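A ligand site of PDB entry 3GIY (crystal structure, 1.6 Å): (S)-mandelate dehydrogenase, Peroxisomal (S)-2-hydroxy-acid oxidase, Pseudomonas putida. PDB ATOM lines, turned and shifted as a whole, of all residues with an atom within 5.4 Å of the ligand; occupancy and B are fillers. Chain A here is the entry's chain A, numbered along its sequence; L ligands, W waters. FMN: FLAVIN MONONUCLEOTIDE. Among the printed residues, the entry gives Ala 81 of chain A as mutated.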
ATOM      1  N   TYR A  26     -15.940 -27.858   1.266  1.00  0.00           N
ATOM      2  CA  TYR A  26     -15.923 -26.484   1.778  1.00  0.00           C
ATOM      3  C   TYR A  26     -14.464 -26.043   1.969  1.00  0.00           C
ATOM      4  O   TYR A  26     -14.112 -24.900   1.692  1.00  0.00           O
ATOM      5  CB  TYR A  26     -16.647 -26.401   3.122  1.00  0.00           C
ATOM      6  CG  TYR A  26     -16.270 -25.179   3.933  1.00  0.00           C
ATOM      7  CD1 TYR A  26     -16.584 -23.891   3.503  1.00  0.00           C
ATOM      8  CD2 TYR A  26     -15.548 -25.311   5.127  1.00  0.00           C
ATOM      9  CE1 TYR A  26     -16.191 -22.769   4.237  1.00  0.00           C
ATOM     10  CE2 TYR A  26     -15.156 -24.188   5.861  1.00  0.00           C
ATOM     11  CZ  TYR A  26     -15.474 -22.926   5.408  1.00  0.00           C
ATOM     12  OH  TYR A  26     -15.078 -21.831   6.137  1.00  0.00           O
ATOM     13  N   LEU A  27     -13.630 -26.972   2.435  1.00  0.00           N
ATOM     14  CA  LEU A  27     -12.215 -26.707   2.677  1.00  0.00           C
ATOM     15  C   LEU A  27     -11.341 -26.670   1.424  1.00  0.00           C
ATOM     16  O   LEU A  27     -10.594 -25.698   1.196  1.00  0.00           O
ATOM     17  CB  LEU A  27     -11.655 -27.758   3.652  1.00  0.00           C
ATOM     18  CG  LEU A  27     -10.138 -27.903   3.837  1.00  0.00           C
ATOM     19  CD1 LEU A  27      -9.567 -26.669   4.541  1.00  0.00           C
ATOM     20  CD2 LEU A  27      -9.845 -29.177   4.636  1.00  0.00           C
ATOM     21  N   GLY A  78      -2.475 -18.848   9.062  1.00  0.00           N
ATOM     22  CA  GLY A  78      -3.358 -17.769   8.651  1.00  0.00           C
ATOM     23  C   GLY A  78      -4.797 -17.885   9.095  1.00  0.00           C
ATOM     24  O   GLY A  78      -5.223 -18.916   9.608  1.00  0.00           O
ATOM     25  N   PRO A  79      -5.588 -16.817   8.883  1.00  0.00           N
ATOM     26  CA  PRO A  79      -7.001 -16.795   9.270  1.00  0.00           C
ATOM     27  C   PRO A  79      -7.904 -17.641   8.380  1.00  0.00           C
ATOM     28  O   PRO A  79      -7.919 -17.469   7.165  1.00  0.00           O
ATOM     29  CB  PRO A  79      -7.353 -15.309   9.183  1.00  0.00           C
ATOM     30  CG  PRO A  79      -6.505 -14.833   8.051  1.00  0.00           C
ATOM     31  CD  PRO A  79      -5.175 -15.515   8.315  1.00  0.00           C
ATOM     32  N   THR A  80      -8.642 -18.568   8.987  1.00  0.00           N
ATOM     33  CA  THR A  80      -9.596 -19.407   8.252  1.00  0.00           C
ATOM     34  C   THR A  80     -10.867 -19.546   9.094  1.00  0.00           C
ATOM     35  O   THR A  80     -10.816 -19.692  10.314  1.00  0.00           O
ATOM     36  CB  THR A  80      -9.012 -20.818   7.931  1.00  0.00           C
ATOM     37  OG1 THR A  80      -8.549 -21.446   9.133  1.00  0.00           O
ATOM     38  CG2 THR A  80      -7.870 -20.696   6.929  1.00  0.00           C
ATOM     39  N   ALA A  81     -12.022 -19.469   8.435  1.00  0.00           N
ATOM     40  CA  ALA A  81     -13.289 -19.546   9.144  1.00  0.00           C
ATOM     41  C   ALA A  81     -13.847 -20.950   9.298  1.00  0.00           C
ATOM     42  O   ALA A  81     -13.555 -21.847   8.507  1.00  0.00           O
ATOM     43  CB  ALA A  81     -14.325 -18.671   8.427  1.00  0.00           C
ATOM     44  N   SER A 108      -9.848 -15.754  12.766  1.00  0.00           N
ATOM     45  CA  SER A 108     -10.799 -15.227  11.802  1.00  0.00           C
ATOM     46  C   SER A 108     -11.956 -14.518  12.480  1.00  0.00           C
ATOM     47  O   SER A 108     -12.288 -14.815  13.632  1.00  0.00           O
ATOM     48  CB  SER A 108     -11.348 -16.377  10.945  1.00  0.00           C
ATOM     49  OG  SER A 108     -12.458 -15.950  10.162  1.00  0.00           O
ATOM     50  N   THR A 109     -12.579 -13.571  11.771  1.00  0.00           N
ATOM     51  CA  THR A 109     -13.724 -12.864  12.315  1.00  0.00           C
ATOM     52  C   THR A 109     -14.888 -13.866  12.346  1.00  0.00           C
ATOM     53  O   THR A 109     -15.849 -13.703  13.095  1.00  0.00           O
ATOM     54  CB  THR A 109     -14.114 -11.660  11.424  1.00  0.00           C
ATOM     55  OG1 THR A 109     -13.243 -10.564  11.704  1.00  0.00           O
ATOM     56  CG2 THR A 109     -15.558 -11.232  11.678  1.00  0.00           C
ATOM     57  N   ALA A 110     -14.764 -14.897  11.518  1.00  0.00           N
ATOM     58  CA  ALA A 110     -15.776 -15.947  11.424  1.00  0.00           C
ATOM     59  C   ALA A 110     -15.303 -17.256  12.085  1.00  0.00           C
ATOM     60  O   ALA A 110     -15.605 -18.350  11.614  1.00  0.00           O
ATOM     61  CB  ALA A 110     -16.131 -16.198   9.961  1.00  0.00           C
ATOM     62  N   GLN A 129      -7.852 -11.256  12.442  1.00  0.00           N
ATOM     63  CA  GLN A 129      -8.204 -10.936  11.076  1.00  0.00           C
ATOM     64  C   GLN A 129      -9.587 -10.315  11.087  1.00  0.00           C
ATOM     65  O   GLN A 129     -10.550 -10.947  11.542  1.00  0.00           O
ATOM     66  CB  GLN A 129      -8.207 -12.196  10.212  1.00  0.00           C
ATOM     67  CG  GLN A 129      -8.746 -12.016   8.784  1.00  0.00           C
ATOM     68  CD  GLN A 129     -10.260 -12.235   8.683  1.00  0.00           C
ATOM     69  OE1 GLN A 129     -10.975 -11.422   8.080  1.00  0.00           O
ATOM     70  NE2 GLN A 129     -10.729 -13.338   9.236  1.00  0.00           N
ATOM     71  N   TYR A 131     -13.026  -8.656   9.300  1.00  0.00           N
ATOM     72  CA  TYR A 131     -13.926  -8.609   8.150  1.00  0.00           C
ATOM     73  C   TYR A 131     -14.901  -7.511   8.562  1.00  0.00           C
ATOM     74  O   TYR A 131     -15.410  -7.524   9.696  1.00  0.00           O
ATOM     75  CB  TYR A 131     -14.731  -9.908   7.994  1.00  0.00           C
ATOM     76  CG  TYR A 131     -14.099 -10.992   7.142  1.00  0.00           C
ATOM     77  CD1 TYR A 131     -13.537 -10.703   5.895  1.00  0.00           C
ATOM     78  CD2 TYR A 131     -14.175 -12.323   7.543  1.00  0.00           C
ATOM     79  CE1 TYR A 131     -13.055 -11.726   5.064  1.00  0.00           C
ATOM     80  CE2 TYR A 131     -13.701 -13.350   6.727  1.00  0.00           C
ATOM     81  CZ  TYR A 131     -13.154 -13.050   5.489  1.00  0.00           C
ATOM     82  OH  TYR A 131     -12.728 -14.079   4.689  1.00  0.00           O
ATOM     83  N   THR A 156      -8.870  -8.050   6.005  1.00  0.00           N
ATOM     84  CA  THR A 156      -9.059  -8.815   4.772  1.00  0.00           C
ATOM     85  C   THR A 156      -9.964  -8.019   3.847  1.00  0.00           C
ATOM     86  O   THR A 156     -11.122  -7.742   4.154  1.00  0.00           O
ATOM     87  CB  THR A 156      -9.683 -10.195   5.058  1.00  0.00           C
ATOM     88  OG1 THR A 156      -8.814 -10.921   5.931  1.00  0.00           O
ATOM     89  CG2 THR A 156      -9.862 -10.969   3.761  1.00  0.00           C
ATOM     90  N   LYS A 231      -4.625  -7.488   4.002  1.00  0.00           N
ATOM     91  CA  LYS A 231      -4.584  -8.779   3.329  1.00  0.00           C
ATOM     92  C   LYS A 231      -5.493  -8.863   2.101  1.00  0.00           C
ATOM     93  O   LYS A 231      -6.568  -8.262   2.065  1.00  0.00           O
ATOM     94  CB  LYS A 231      -4.957  -9.870   4.347  1.00  0.00           C
ATOM     95  CG  LYS A 231      -5.042 -11.301   3.821  1.00  0.00           C
ATOM     96  CD  LYS A 231      -5.172 -12.278   4.993  1.00  0.00           C
ATOM     97  CE  LYS A 231      -5.294 -13.728   4.543  1.00  0.00           C
ATOM     98  NZ  LYS A 231      -6.659 -14.083   4.045  1.00  0.00           N
ATOM     99  N   SER A 253      -2.266 -11.944  -1.465  1.00  0.00           N
ATOM    100  CA  SER A 253      -3.068 -13.151  -1.417  1.00  0.00           C
ATOM    101  C   SER A 253      -4.256 -13.146  -2.376  1.00  0.00           C
ATOM    102  O   SER A 253      -4.785 -12.084  -2.699  1.00  0.00           O
ATOM    103  CB  SER A 253      -3.591 -13.325   0.017  1.00  0.00           C
ATOM    104  OG  SER A 253      -4.620 -14.289   0.103  1.00  0.00           O
ATOM    105  N   HIS A 255      -6.702 -15.338  -1.637  1.00  0.00           N
ATOM    106  CA  HIS A 255      -7.593 -16.097  -0.765  1.00  0.00           C
ATOM    107  C   HIS A 255      -7.616 -17.580  -1.089  1.00  0.00           C
ATOM    108  O   HIS A 255      -8.664 -18.224  -1.015  1.00  0.00           O
ATOM    109  CB  HIS A 255      -9.021 -15.528  -0.895  1.00  0.00           C
ATOM    110  CG  HIS A 255      -9.838 -15.650   0.351  1.00  0.00           C
ATOM    111  ND1 HIS A 255     -10.151 -14.550   1.131  1.00  0.00           N
ATOM    112  CD2 HIS A 255     -10.439 -16.713   0.936  1.00  0.00           C
ATOM    113  CE1 HIS A 255     -10.916 -14.939   2.135  1.00  0.00           C
ATOM    114  NE2 HIS A 255     -11.107 -16.242   2.039  1.00  0.00           N
ATOM    115  N   GLY A 256      -6.451 -18.123  -1.443  1.00  0.00           N
ATOM    116  CA  GLY A 256      -6.352 -19.537  -1.770  1.00  0.00           C
ATOM    117  C   GLY A 256      -7.216 -19.950  -2.956  1.00  0.00           C
ATOM    118  O   GLY A 256      -7.726 -21.065  -2.980  1.00  0.00           O
ATOM    119  N   ARG A 258     -10.127 -18.978  -3.722  1.00  0.00           N
ATOM    120  CA  ARG A 258     -11.534 -19.141  -3.347  1.00  0.00           C
ATOM    121  C   ARG A 258     -12.443 -17.971  -3.688  1.00  0.00           C
ATOM    122  O   ARG A 258     -13.664 -18.073  -3.537  1.00  0.00           O
ATOM    123  CB  ARG A 258     -11.627 -19.420  -1.843  1.00  0.00           C
ATOM    124  CG  ARG A 258     -10.952 -20.701  -1.407  1.00  0.00           C
ATOM    125  CD  ARG A 258     -10.698 -20.717   0.083  1.00  0.00           C
ATOM    126  NE  ARG A 258     -11.911 -20.827   0.896  1.00  0.00           N
ATOM    127  CZ  ARG A 258     -12.619 -21.938   1.040  1.00  0.00           C
ATOM    128  NH1 ARG A 258     -12.247 -23.051   0.410  1.00  0.00           N
ATOM    129  NH2 ARG A 258     -13.678 -21.952   1.847  1.00  0.00           N
ATOM    130  N   ASP A 284       0.532 -15.603   0.985  1.00  0.00           N
ATOM    131  CA  ASP A 284      -0.076 -16.917   1.132  1.00  0.00           C
ATOM    132  C   ASP A 284      -0.725 -17.302  -0.194  1.00  0.00           C
ATOM    133  O   ASP A 284      -0.618 -16.541  -1.169  1.00  0.00           O
ATOM    134  CB  ASP A 284      -1.131 -16.930   2.271  1.00  0.00           C
ATOM    135  CG  ASP A 284      -2.393 -16.151   1.933  1.00  0.00           C
ATOM    136  OD1 ASP A 284      -2.726 -15.994   0.744  1.00  0.00           O
ATOM    137  OD2 ASP A 284      -3.074 -15.696   2.881  1.00  0.00           O
ATOM    138  N   SER A 285      -1.356 -18.467  -0.237  1.00  0.00           N
ATOM    139  CA  SER A 285      -2.067 -18.993  -1.405  1.00  0.00           C
ATOM    140  C   SER A 285      -1.259 -19.962  -2.274  1.00  0.00           C
ATOM    141  O   SER A 285      -0.459 -19.547  -3.122  1.00  0.00           O
ATOM    142  CB  SER A 285      -2.617 -17.852  -2.272  1.00  0.00           C
ATOM    143  OG  SER A 285      -3.590 -17.085  -1.575  1.00  0.00           O
ATOM    144  N   GLY A 286      -1.476 -21.258  -2.044  1.00  0.00           N
ATOM    145  CA  GLY A 286      -0.798 -22.280  -2.811  1.00  0.00           C
ATOM    146  C   GLY A 286       0.397 -22.972  -2.174  1.00  0.00           C
ATOM    147  O   GLY A 286       0.912 -23.931  -2.740  1.00  0.00           O
ATOM    148  N   PHE A 287       0.833 -22.502  -0.996  1.00  0.00           N
ATOM    149  CA  PHE A 287       1.991 -23.108  -0.340  1.00  0.00           C
ATOM    150  C   PHE A 287       1.717 -24.485   0.269  1.00  0.00           C
ATOM    151  O   PHE A 287       0.812 -24.636   1.102  1.00  0.00           O
ATOM    152  CB  PHE A 287       2.567 -22.153   0.722  1.00  0.00           C
ATOM    153  CG  PHE A 287       3.061 -20.854   0.154  1.00  0.00           C
ATOM    154  CD1 PHE A 287       2.175 -19.811  -0.110  1.00  0.00           C
ATOM    155  CD2 PHE A 287       4.405 -20.701  -0.175  1.00  0.00           C
ATOM    156  CE1 PHE A 287       2.633 -18.614  -0.704  1.00  0.00           C
ATOM    157  CE2 PHE A 287       4.875 -19.510  -0.764  1.00  0.00           C
ATOM    158  CZ  PHE A 287       3.971 -18.469  -1.031  1.00  0.00           C
ATOM    159  N   ARG A 288       2.494 -25.486  -0.148  1.00  0.00           N
ATOM    160  CA  ARG A 288       2.341 -26.858   0.336  1.00  0.00           C
ATOM    161  C   ARG A 288       3.684 -27.513   0.700  1.00  0.00           C
ATOM    162  O   ARG A 288       3.759 -28.278   1.677  1.00  0.00           O
ATOM    163  CB  ARG A 288       1.636 -27.700  -0.733  1.00  0.00           C
ATOM    164  CG  ARG A 288       0.269 -27.176  -1.155  1.00  0.00           C
ATOM    165  CD  ARG A 288      -0.792 -27.339  -0.065  1.00  0.00           C
ATOM    166  NE  ARG A 288      -2.104 -26.930  -0.531  1.00  0.00           N
ATOM    167  CZ  ARG A 288      -2.519 -25.666  -0.607  1.00  0.00           C
ATOM    168  NH1 ARG A 288      -1.724 -24.679  -0.228  1.00  0.00           N
ATOM    169  NH2 ARG A 288      -3.730 -25.388  -1.064  1.00  0.00           N
ATOM    170  N   LEU A 305       1.979 -17.339   5.185  1.00  0.00           N
ATOM    171  CA  LEU A 305       0.852 -17.787   6.004  1.00  0.00           C
ATOM    172  C   LEU A 305       0.332 -19.087   5.413  1.00  0.00           C
ATOM    173  O   LEU A 305       0.203 -19.228   4.193  1.00  0.00           O
ATOM    174  CB  LEU A 305      -0.281 -16.764   6.037  1.00  0.00           C
ATOM    175  CG  LEU A 305       0.036 -15.411   6.689  1.00  0.00           C
ATOM    176  CD1 LEU A 305       0.594 -14.453   5.633  1.00  0.00           C
ATOM    177  CD2 LEU A 305      -1.234 -14.834   7.322  1.00  0.00           C
ATOM    178  N   LEU A 306       0.049 -20.037   6.294  1.00  0.00           N
ATOM    179  CA  LEU A 306      -0.472 -21.319   5.878  1.00  0.00           C
ATOM    180  C   LEU A 306      -1.995 -21.285   5.971  1.00  0.00           C
ATOM    181  O   LEU A 306      -2.564 -20.733   6.913  1.00  0.00           O
ATOM    182  CB  LEU A 306       0.071 -22.437   6.773  1.00  0.00           C
ATOM    183  CG  LEU A 306       1.595 -22.574   6.806  1.00  0.00           C
ATOM    184  CD1 LEU A 306       1.982 -23.725   7.716  1.00  0.00           C
ATOM    185  CD2 LEU A 306       2.113 -22.811   5.387  1.00  0.00           C
ATOM    186  N   GLY A 307      -2.640 -21.871   4.977  1.00  0.00           N
ATOM    187  CA  GLY A 307      -4.081 -21.933   4.979  1.00  0.00           C
ATOM    188  C   GLY A 307      -4.481 -23.384   5.086  1.00  0.00           C
ATOM    189  O   GLY A 307      -4.509 -23.953   6.177  1.00  0.00           O
ATOM    190  N   ARG A 308      -4.744 -24.011   3.944  1.00  0.00           N
ATOM    191  CA  ARG A 308      -5.164 -25.406   3.931  1.00  0.00           C
ATOM    192  C   ARG A 308      -4.107 -26.379   4.488  1.00  0.00           C
ATOM    193  O   ARG A 308      -4.468 -27.378   5.107  1.00  0.00           O
ATOM    194  CB  ARG A 308      -5.555 -25.829   2.503  1.00  0.00           C
ATOM    195  CG  ARG A 308      -6.750 -25.079   1.907  1.00  0.00           C
ATOM    196  CD  ARG A 308      -7.200 -25.747   0.611  1.00  0.00           C
ATOM    197  NE  ARG A 308      -8.249 -25.036  -0.129  1.00  0.00           N
ATOM    198  CZ  ARG A 308      -8.050 -23.939  -0.854  1.00  0.00           C
ATOM    199  NH1 ARG A 308      -6.838 -23.403  -0.963  1.00  0.00           N
ATOM    200  NH2 ARG A 308      -9.053 -23.395  -1.522  1.00  0.00           N
ATOM    201  N   ALA A 309      -2.827 -26.102   4.265  1.00  0.00           N
ATOM    202  CA  ALA A 309      -1.763 -26.992   4.735  1.00  0.00           C
ATOM    203  C   ALA A 309      -1.969 -27.469   6.166  1.00  0.00           C
ATOM    204  O   ALA A 309      -2.037 -28.670   6.426  1.00  0.00           O
ATOM    205  CB  ALA A 309      -0.403 -26.300   4.607  1.00  0.00           C
ATOM    206  N   LEU A 311      -4.634 -26.960   7.937  1.00  0.00           N
ATOM    207  CA  LEU A 311      -6.018 -27.380   8.144  1.00  0.00           C
ATOM    208  C   LEU A 311      -6.151 -28.880   7.867  1.00  0.00           C
ATOM    209  O   LEU A 311      -6.999 -29.551   8.460  1.00  0.00           O
ATOM    210  CB  LEU A 311      -6.978 -26.595   7.236  1.00  0.00           C
ATOM    211  CG  LEU A 311      -7.261 -25.135   7.637  1.00  0.00           C
ATOM    212  CD1 LEU A 311      -8.367 -24.578   6.750  1.00  0.00           C
ATOM    213  CD2 LEU A 311      -7.680 -25.054   9.110  1.00  0.00           C
HETATM  214  N1  FMN L   1      -9.139 -15.571   4.951  1.00  0.00           N
HETATM  215  C2  FMN L   1      -9.456 -14.573   5.848  1.00  0.00           C
HETATM  216  O2  FMN L   1      -8.879 -13.554   5.893  1.00  0.00           O
HETATM  217  N3  FMN L   1     -10.569 -14.851   6.771  1.00  0.00           N
HETATM  218  C4  FMN L   1     -11.349 -16.057   6.829  1.00  0.00           C
HETATM  219  O4  FMN L   1     -12.258 -16.237   7.626  1.00  0.00           O
HETATM  220  C4A FMN L   1     -10.959 -17.130   5.849  1.00  0.00           C
HETATM  221  N5  FMN L   1     -11.553 -18.356   5.848  1.00  0.00           N
HETATM  222  C5A FMN L   1     -11.079 -19.401   5.054  1.00  0.00           C
HETATM  223  C6  FMN L   1     -11.642 -20.735   5.184  1.00  0.00           C
HETATM  224  C7  FMN L   1     -11.105 -21.910   4.467  1.00  0.00           C
HETATM  225  C7M FMN L   1     -11.731 -23.265   4.699  1.00  0.00           C
HETATM  226  C8  FMN L   1      -9.902 -21.707   3.509  1.00  0.00           C
HETATM  227  C8M FMN L   1      -9.241 -22.816   2.730  1.00  0.00           C
HETATM  228  C9  FMN L   1      -9.374 -20.387   3.384  1.00  0.00           C
HETATM  229  C9A FMN L   1      -9.881 -19.190   4.122  1.00  0.00           C
HETATM  230  N10 FMN L   1      -9.326 -17.822   4.115  1.00  0.00           N
HETATM  231  C10 FMN L   1      -9.784 -16.753   4.949  1.00  0.00           C
HETATM  232  C1' FMN L   1      -8.155 -17.564   3.261  1.00  0.00           C
HETATM  233  C2' FMN L   1      -6.840 -17.843   3.992  1.00  0.00           C
HETATM  234  O2' FMN L   1      -6.537 -16.872   4.920  1.00  0.00           O
HETATM  235  C3' FMN L   1      -5.655 -17.959   3.055  1.00  0.00           C
HETATM  236  O3' FMN L   1      -5.612 -16.745   2.211  1.00  0.00           O
HETATM  237  C4' FMN L   1      -5.692 -19.083   2.019  1.00  0.00           C
HETATM  238  O4' FMN L   1      -6.201 -20.301   2.535  1.00  0.00           O
HETATM  239  C5' FMN L   1      -4.288 -19.312   1.533  1.00  0.00           C
HETATM  240  O5' FMN L   1      -4.185 -20.390   0.551  1.00  0.00           O
HETATM  241  P   FMN L   1      -3.936 -21.900   0.727  1.00  0.00           P
HETATM  242  O1P FMN L   1      -3.547 -22.510  -0.581  1.00  0.00           O
HETATM  243  O2P FMN L   1      -5.212 -22.446   1.297  1.00  0.00           O
HETATM  244  O3P FMN L   1      -2.814 -21.947   1.741  1.00  0.00           O
HETATM  245  O   HOH W   1     -11.792 -23.989   7.988  1.00  0.00           O
HETATM  246  O   HOH W   2     -14.223 -16.481   5.071  1.00  0.00           O
HETATM  247  O   HOH W   3      -0.601 -20.407   1.807  1.00  0.00           O
HETATM  248  O   HOH W   4      -4.614 -21.993  -3.253  1.00  0.00           O
HETATM  249  O   HOH W   5     -14.388 -19.656   3.867  1.00  0.00           O
HETATM  250  O   HOH W   6      -1.252 -23.867   3.108  1.00  0.00           O
HETATM  251  O   HOH W   7      -3.699 -16.807   5.532  1.00  0.00           O
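The side-chain hydroxyl of Ser 108 sits at hydrogen-bond distance from an oxygen (O4) of the ligand.
OG1 of Thr 156 sits at hydrogen-bond distance from O2 of the ligand, 2.6 Å away.
The backbone carbonyl oxygen of Pro 79 sits at hydrogen-bond distance from an oxygen (O2') of the ligand (2.7 Å).
An oxygen (O3') of the ligand sits at hydrogen-bond distance from the side-chain carboxylate (OD2) of Asp 284, 2.8 Å away.
An oxygen (O1P) of the ligand lies within hydrogen-bond range of the backbone NH (N) of Gly 286 (2.8 Å).
NH1 of Arg 288 is in salt-bridge range of O1P of the ligand (2.9 Å).
N of Ala 81 is in hydrogen-bond range of N5 of the ligand (2.9 Å).
The side-chain amide nitrogen (NE2) of Gln 129 lies close to a nitrogen (N3) of the ligand (2.9 Å).
O2' of the ligand lies within hydrogen-bond range of NZ of Lys 231, at 2.9 Å.
The backbone NH of Arg 308 lies close to an oxygen (O2P) of the ligand, at 3.1 Å.
NH1 of Arg 308 lies within salt-bridge range of O2P of the ligand, at 2.9 Å.
OH of Tyr 131 lies within hydrogen-bond range of N3 of the ligand (3.1 Å).
An oxygen (O3P) of the ligand is in hydrogen-bond range of the backbone NH of Gly 307, at 3.2 Å.
The side-chain hydroxyl of Ser 253 lies within hydrogen-bond range of an oxygen (O3') of the ligand (3.4 Å).
The side-chain hydroxyl of Ser 108 lies close to the side-chain amide nitrogen of Gln 129 (3.3 Å).
The side-chain hydroxyl of Tyr 26 is in hydrogen-bond range of the backbone carbonyl oxygen of Ala 81 (2.8 Å).
The backbone carbonyl oxygen (O) of Gln 129 is in hydrogen-bond range of the side-chain hydroxyl (OG1) of Thr 109 (2.7 Å).
The guanidinium group (NE) of Arg 308 lies within hydrogen-bond range of the backbone carbonyl oxygen (O) of Leu 27 (2.8 Å).
The backbone NH of Gly 256 lies within hydrogen-bond range of the side-chain hydroxyl of Ser 285, 3.0 Å away.
OG of Ser 285 lies within hydrogen-bond range of OG of Ser 253.
The guanidinium group of Arg 258 is in hydrogen-bond range of the backbone carbonyl oxygen of Leu 27 (3.2 Å).
O of Tyr 26 is in hydrogen-bond range of NH1 of Arg 258 (2.9 Å).
NE2 of His 255 sits close to N10 of the ligand.
Merely in contact with the ligand: Tyr 26 (3.7 Å), Leu 27 (3.5 Å), Thr 80 (3.3 Å), Gly 256 (3.3 Å), Arg 258 (3.4 Å) and Ser 285 (3.2 Å).
20 residues have an atom within 4 Å of the ligand: Tyr 26, Leu 27, Pro 79, Thr 80, Ala 81, Ser 108, Gln 129, Tyr 131, Thr 156, Lys 231, Ser 253, His 255, Gly 256, Arg 258, Asp 284, Ser 285, Gly 286, Arg 288, Gly 307 and Arg 308.
Along chain A the residues within 4 Å of the ligand span positions 26 to 308.
Water W3 lies within hydrogen-bond range of an oxygen (O3P) of the ligand (2.7 Å), the backbone carbonyl oxygen of Leu 305 (2.8 Å) and the backbone NH of Ser 285 (2.9 Å).
Water W7 lies within hydrogen-bond range of O2' of the ligand (2.9 Å) and OD2 of Asp 284 (2.9 Å).
Water W4 lies within hydrogen-bond range of an oxygen (O1P) of the ligand (2.9 Å), the backbone carbonyl oxygen of Gly 256 (3.3 Å), the backbone NH of Gly 286 (3.4 Å) and the guanidinium group of Arg 308 (3.5 Å).
Water W5 bridges the guanidinium group (NH2) of Arg 258 (3.1 Å) and the side-chain hydroxyl (OH) of Tyr 26 (3.2 Å).
Water W2 lies within hydrogen-bond range of the side-chain hydroxyl (OH) of Tyr 131 (2.9 Å) and an oxygen (O4) of the ligand (3.2 Å).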
